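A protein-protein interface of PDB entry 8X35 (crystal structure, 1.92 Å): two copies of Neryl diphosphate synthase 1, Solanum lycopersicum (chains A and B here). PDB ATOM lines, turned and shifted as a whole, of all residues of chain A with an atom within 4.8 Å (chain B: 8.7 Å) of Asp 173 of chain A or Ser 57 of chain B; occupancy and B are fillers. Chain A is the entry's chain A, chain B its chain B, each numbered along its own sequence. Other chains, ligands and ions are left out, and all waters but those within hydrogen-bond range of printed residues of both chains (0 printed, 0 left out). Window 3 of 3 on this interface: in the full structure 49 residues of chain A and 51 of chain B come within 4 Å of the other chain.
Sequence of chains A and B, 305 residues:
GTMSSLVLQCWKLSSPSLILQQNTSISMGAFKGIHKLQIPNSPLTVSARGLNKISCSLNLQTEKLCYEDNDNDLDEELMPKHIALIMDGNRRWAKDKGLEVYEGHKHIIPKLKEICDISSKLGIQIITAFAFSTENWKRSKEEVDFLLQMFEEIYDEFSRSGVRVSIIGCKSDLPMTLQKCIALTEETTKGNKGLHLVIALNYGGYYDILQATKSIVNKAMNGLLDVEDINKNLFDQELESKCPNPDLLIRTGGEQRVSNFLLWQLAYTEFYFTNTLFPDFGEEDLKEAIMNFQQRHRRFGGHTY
The side-chain sulfur (SG) of Cys 56 of chain B forms a disulfide with the side-chain sulfur (SG) of Cys 170 of chain A (2.0 Å). The backbone carbonyl oxygen of Cys 56 of chain B is in hydrogen-bond range of the side-chain hydroxyl of Ser 172 of chain A (3.2 Å). OD1 of Asp 173 of chain A lies within hydrogen-bond range of OG of Ser 57 of chain B (3.4 Å). The side-chain carboxylate (OD2) of Asp 173 of chain A is in hydrogen-bond range of the backbone NH (N) of Leu 58 of chain B (2.8 Å).
OD1 of Asn 202 of chain A lies within hydrogen-bond range of NE1 of Trp 137 of chain A, 2.9 Å away. SG of Cys 170 of chain A sits at hydrogen-bond distance from OG of Ser 172 of chain A, 3.7 Å away. O of Cys 170 of chain A lies within hydrogen-bond range of ND2 of Asn 202 of chain A. The side-chain amide nitrogen of Asn 202 of chain A lies within hydrogen-bond range of the side-chain carboxylate of Asp 173 of chain A (3.3 Å).
Among the printed residues, merely in contact across the chains: Trp 137 of chain A with Asn 59 of chain B, Cys 170 of chain A with Leu 58 of chain B, Asn 202 of chain A with Leu 58 of chain B, Trp 137 of chain A with Leu 58 of chain B, Asp 173 of chain A with Asn 59 of chain B and Cys 170 of chain A with Ser 57 of chain B.
Printed residues of chain A within 4 Å of Ser 57 of chain B: Cys 170 and Asp 173. Of chain B, only Cys 56 (3.2 Å) comes within 4 Å of Ser 172 of chain A. Of the printed residues of chain A, Cys 56 of chain B touches Cys 170 (2.0 Å) and Ser 172 (3.2 Å). Of the printed residues of chain A, Leu 58 of chain B touches Trp 137, Cys 170, Asp 173 and Asn 202. Of the printed residues of chain A, Asn 59 of chain B touches Trp 137 and Asp 173. Printed residues of chain B within 4 Å of Cys 170 of chain A: Cys 56, Ser 57 and Leu 58. Lys 64 of chain B touches none of the printed residues of chain A. Pro 175 of chain A touches none of the printed residues of chain B. The nearest residue of chain B that does not touch Asp 173 of chain A is Cys 56 of chain B (4.5 Å). The nearest printed residue of chain A that does not touch Ser 57 of chain B is Ser 172 of chain A (5.2 Å).
Of the 9 printed residues of chain B, 4 touch a printed residue of chain A. Of the 8 printed residues of chain A, 5 touch a printed residue of chain B. Printed residues of chain A that touch a printed residue of chain B: Trp 137, Cys 170, Ser 172, Asp 173 and Asn 202. Hydrophobic or aromatic side chains of chain A within 4 Å of the printed part of chain B: Trp 137. Along chain A the printed residues that touch a printed residue of chain B span positions 137 to 202. Among the printed residues, no Asp or Glu carboxylate lies within 4 Å of a Lys or Arg side-chain nitrogen of the other chain.
No position is printed for both chains. Of the 10 pairs that touch across the chains among the printed residues, none has its exchanged pair printed and touching as well.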
ATOM      1  N   TRP A 137     -16.393 -24.413  12.898  1.00  0.00           N
ATOM      2  CA  TRP A 137     -17.330 -23.986  13.929  1.00  0.00           C
ATOM      3  C   TRP A 137     -18.604 -23.384  13.340  1.00  0.00           C
ATOM      4  O   TRP A 137     -19.583 -23.203  14.073  1.00  0.00           O
ATOM      5  CB  TRP A 137     -16.653 -22.956  14.845  1.00  0.00           C
ATOM      6  CG  TRP A 137     -15.538 -23.483  15.720  1.00  0.00           C
ATOM      7  CD1 TRP A 137     -14.202 -23.256  15.552  1.00  0.00           C
ATOM      8  CD2 TRP A 137     -15.664 -24.226  16.949  1.00  0.00           C
ATOM      9  NE1 TRP A 137     -13.485 -23.865  16.556  1.00  0.00           N
ATOM     10  CE2 TRP A 137     -14.357 -24.456  17.432  1.00  0.00           C
ATOM     11  CE3 TRP A 137     -16.748 -24.739  17.671  1.00  0.00           C
ATOM     12  CZ2 TRP A 137     -14.104 -25.167  18.609  1.00  0.00           C
ATOM     13  CZ3 TRP A 137     -16.493 -25.455  18.843  1.00  0.00           C
ATOM     14  CH2 TRP A 137     -15.181 -25.663  19.294  1.00  0.00           C
ATOM     15  N   CYS A 170      -5.745 -24.925  18.917  1.00  0.00           N
ATOM     16  CA  CYS A 170      -6.083 -24.255  20.180  1.00  0.00           C
ATOM     17  C   CYS A 170      -6.931 -25.203  21.022  1.00  0.00           C
ATOM     18  O   CYS A 170      -8.155 -25.266  20.872  1.00  0.00           O
ATOM     19  CB  CYS A 170      -6.818 -22.945  19.924  1.00  0.00           C
ATOM     20  SG  CYS A 170      -7.343 -22.071  21.455  1.00  0.00           S
ATOM     21  N   LYS A 171      -6.268 -25.957  21.901  1.00  0.00           N
ATOM     22  CA  LYS A 171      -6.935 -26.965  22.717  1.00  0.00           C
ATOM     23  C   LYS A 171      -7.907 -26.374  23.738  1.00  0.00           C
ATOM     24  O   LYS A 171      -8.865 -27.048  24.125  1.00  0.00           O
ATOM     25  CB  LYS A 171      -5.878 -27.813  23.430  1.00  0.00           C
ATOM     26  CG  LYS A 171      -5.033 -28.671  22.497  1.00  0.00           C
ATOM     27  CD  LYS A 171      -3.766 -29.162  23.191  1.00  0.00           C
ATOM     28  CE  LYS A 171      -3.033 -30.196  22.337  1.00  0.00           C
ATOM     29  NZ  LYS A 171      -1.601 -30.472  22.698  1.00  0.00           N
ATOM     30  N   SER A 172      -7.713 -25.128  24.162  1.00  0.00           N
ATOM     31  CA  SER A 172      -8.536 -24.605  25.251  1.00  0.00           C
ATOM     32  C   SER A 172      -9.981 -24.330  24.836  1.00  0.00           C
ATOM     33  O   SER A 172     -10.841 -24.206  25.713  1.00  0.00           O
ATOM     34  CB  SER A 172      -7.896 -23.349  25.832  1.00  0.00           C
ATOM     35  OG  SER A 172      -8.175 -22.220  25.026  1.00  0.00           O
ATOM     36  N   ASP A 173     -10.280 -24.248  23.529  1.00  0.00           N
ATOM     37  CA  ASP A 173     -11.662 -24.129  23.074  1.00  0.00           C
ATOM     38  C   ASP A 173     -12.408 -25.449  23.083  1.00  0.00           C
ATOM     39  O   ASP A 173     -13.616 -25.465  22.811  1.00  0.00           O
ATOM     40  CB  ASP A 173     -11.732 -23.582  21.647  1.00  0.00           C
ATOM     41  CG  ASP A 173     -11.362 -22.130  21.553  1.00  0.00           C
ATOM     42  OD1 ASP A 173     -11.859 -21.324  22.363  1.00  0.00           O
ATOM     43  OD2 ASP A 173     -10.574 -21.796  20.646  1.00  0.00           O
ATOM     44  N   LEU A 174     -11.731 -26.535  23.325  1.00  0.00           N
ATOM     45  CA  LEU A 174     -12.408 -27.806  23.216  1.00  0.00           C
ATOM     46  C   LEU A 174     -13.034 -28.172  24.558  1.00  0.00           C
ATOM     47  O   LEU A 174     -12.675 -27.605  25.592  1.00  0.00           O
ATOM     48  CB  LEU A 174     -11.410 -28.873  22.760  1.00  0.00           C
ATOM     49  CG  LEU A 174     -10.707 -28.573  21.429  1.00  0.00           C
ATOM     50  CD1 LEU A 174      -9.638 -29.598  21.167  1.00  0.00           C
ATOM     51  CD2 LEU A 174     -11.715 -28.549  20.279  1.00  0.00           C
ATOM     52  N   PRO A 175     -14.018 -29.070  24.568  1.00  0.00           N
ATOM     53  CA  PRO A 175     -14.541 -29.579  25.844  1.00  0.00           C
ATOM     54  C   PRO A 175     -13.440 -30.172  26.713  1.00  0.00           C
ATOM     55  O   PRO A 175     -12.526 -30.845  26.232  1.00  0.00           O
ATOM     56  CB  PRO A 175     -15.553 -30.643  25.408  1.00  0.00           C
ATOM     57  CG  PRO A 175     -16.008 -30.166  24.054  1.00  0.00           C
ATOM     58  CD  PRO A 175     -14.790 -29.562  23.414  1.00  0.00           C
ATOM     59  N   ASN A 202      -8.980 -28.041  15.638  1.00  0.00           N
ATOM     60  CA  ASN A 202      -9.173 -26.600  15.885  1.00  0.00           C
ATOM     61  C   ASN A 202      -7.938 -25.793  15.480  1.00  0.00           C
ATOM     62  O   ASN A 202      -7.426 -24.947  16.229  1.00  0.00           O
ATOM     63  CB  ASN A 202      -9.562 -26.302  17.337  1.00  0.00           C
ATOM     64  CG  ASN A 202     -10.096 -24.877  17.520  1.00  0.00           C
ATOM     65  OD1 ASN A 202     -10.661 -24.277  16.599  1.00  0.00           O
ATOM     66  ND2 ASN A 202      -9.956 -24.353  18.721  1.00  0.00           N
ATOM     67  N   SER B  55      -2.478 -17.105  25.425  1.00  0.00           N
ATOM     68  CA  SER B  55      -3.857 -17.587  25.485  1.00  0.00           C
ATOM     69  C   SER B  55      -4.517 -17.525  24.094  1.00  0.00           C
ATOM     70  O   SER B  55      -4.212 -16.634  23.302  1.00  0.00           O
ATOM     71  CB  SER B  55      -4.651 -16.768  26.510  1.00  0.00           C
ATOM     72  OG  SER B  55      -5.997 -17.200  26.604  1.00  0.00           O
ATOM     73  N   CYS B  56      -5.406 -18.471  23.784  1.00  0.00           N
ATOM     74  CA  CYS B  56      -6.025 -18.541  22.463  1.00  0.00           C
ATOM     75  C   CYS B  56      -7.527 -18.763  22.584  1.00  0.00           C
ATOM     76  O   CYS B  56      -8.015 -19.344  23.559  1.00  0.00           O
ATOM     77  CB  CYS B  56      -5.405 -19.664  21.589  1.00  0.00           C
ATOM     78  SG  CYS B  56      -5.578 -21.386  22.203  1.00  0.00           S
ATOM     79  N   SER B  57      -8.255 -18.286  21.577  1.00  0.00           N
ATOM     80  CA  SER B  57      -9.692 -18.535  21.490  1.00  0.00           C
ATOM     81  C   SER B  57     -10.123 -18.283  20.056  1.00  0.00           C
ATOM     82  O   SER B  57      -9.984 -17.162  19.553  1.00  0.00           O
ATOM     83  CB  SER B  57     -10.473 -17.652  22.465  1.00  0.00           C
ATOM     84  OG  SER B  57     -11.859 -17.949  22.411  1.00  0.00           O
ATOM     85  N   LEU B  58     -10.639 -19.323  19.399  1.00  0.00           N
ATOM     86  CA  LEU B  58     -10.955 -19.285  17.975  1.00  0.00           C
ATOM     87  C   LEU B  58     -12.403 -19.665  17.703  1.00  0.00           C
ATOM     88  O   LEU B  58     -12.774 -19.883  16.542  1.00  0.00           O
ATOM     89  CB  LEU B  58     -10.020 -20.226  17.211  1.00  0.00           C
ATOM     90  CG  LEU B  58      -8.538 -20.124  17.569  1.00  0.00           C
ATOM     91  CD1 LEU B  58      -7.782 -21.280  16.933  1.00  0.00           C
ATOM     92  CD2 LEU B  58      -7.978 -18.780  17.117  1.00  0.00           C
ATOM     93  N   ASN B  59     -13.225 -19.754  18.746  1.00  0.00           N
ATOM     94  CA  ASN B  59     -14.581 -20.270  18.614  1.00  0.00           C
ATOM     95  C   ASN B  59     -15.523 -19.221  18.038  1.00  0.00           C
ATOM     96  O   ASN B  59     -16.151 -19.438  16.996  1.00  0.00           O
ATOM     97  CB  ASN B  59     -15.080 -20.752  19.979  1.00  0.00           C
ATOM     98  CG  ASN B  59     -16.084 -21.871  19.868  1.00  0.00           C
ATOM     99  OD1 ASN B  59     -16.927 -21.878  18.968  1.00  0.00           O
ATOM    100  ND2 ASN B  59     -16.003 -22.833  20.783  1.00  0.00           N
ATOM    101  N   LEU B  60     -15.626 -18.072  18.705  1.00  0.00           N
ATOM    102  CA  LEU B  60     -16.593 -17.041  18.342  1.00  0.00           C
ATOM    103  C   LEU B  60     -15.993 -16.145  17.259  1.00  0.00           C
ATOM    104  O   LEU B  60     -15.046 -15.394  17.519  1.00  0.00           O
ATOM    105  CB  LEU B  60     -16.997 -16.236  19.577  1.00  0.00           C
ATOM    106  CG  LEU B  60     -17.466 -17.017  20.814  1.00  0.00           C
ATOM    107  CD1 LEU B  60     -18.178 -16.097  21.799  1.00  0.00           C
ATOM    108  CD2 LEU B  60     -18.360 -18.199  20.446  1.00  0.00           C
ATOM    109  N   GLN B  61     -16.555 -16.227  16.052  1.00  0.00           N
ATOM    110  CA  GLN B  61     -16.112 -15.471  14.878  1.00  0.00           C
ATOM    111  C   GLN B  61     -14.592 -15.486  14.728  1.00  0.00           C
ATOM    112  O   GLN B  61     -13.930 -14.471  14.955  1.00  0.00           O
ATOM    113  CB  GLN B  61     -16.614 -14.024  14.942  1.00  0.00           C
ATOM    114  CG  GLN B  61     -16.854 -13.374  13.580  1.00  0.00           C
ATOM    115  CD  GLN B  61     -15.594 -13.242  12.740  1.00  0.00           C
ATOM    116  OE1 GLN B  61     -15.404 -13.974  11.767  1.00  0.00           O
ATOM    117  NE2 GLN B  61     -14.728 -12.304  13.110  1.00  0.00           N
ATOM    118  N   LYS B  64     -14.778 -12.567   8.551  1.00  0.00           N
ATOM    119  CA  LYS B  64     -13.453 -11.975   8.407  1.00  0.00           C
ATOM    120  C   LYS B  64     -12.666 -12.545   7.218  1.00  0.00           C
ATOM    121  O   LYS B  64     -11.438 -12.483   7.210  1.00  0.00           O
ATOM    122  CB  LYS B  64     -12.660 -12.160   9.712  1.00  0.00           C
ATOM    123  CG  LYS B  64     -12.698 -13.578  10.279  1.00  0.00           C
ATOM    124  CD  LYS B  64     -11.384 -13.982  10.944  1.00  0.00           C
ATOM    125  CE  LYS B  64     -11.314 -15.497  11.154  1.00  0.00           C
ATOM    126  NZ  LYS B  64      -9.921 -16.013  11.332  1.00  0.00           N
ATOM    127  N   GLU B 228      -2.759  -8.067  22.378  1.00  0.00           N
ATOM    128  CA  GLU B 228      -4.141  -8.476  22.194  1.00  0.00           C
ATOM    129  C   GLU B 228      -4.778  -7.855  20.959  1.00  0.00           C
ATOM    130  O   GLU B 228      -5.882  -8.261  20.583  1.00  0.00           O
ATOM    131  CB  GLU B 228      -4.968  -8.112  23.430  1.00  0.00           C
ATOM    132  CG  GLU B 228      -4.490  -8.772  24.724  1.00  0.00           C
ATOM    133  CD  GLU B 228      -4.225 -10.270  24.598  1.00  0.00           C
ATOM    134  OE1 GLU B 228      -5.057 -10.989  23.999  1.00  0.00           O
ATOM    135  OE2 GLU B 228      -3.181 -10.729  25.120  1.00  0.00           O
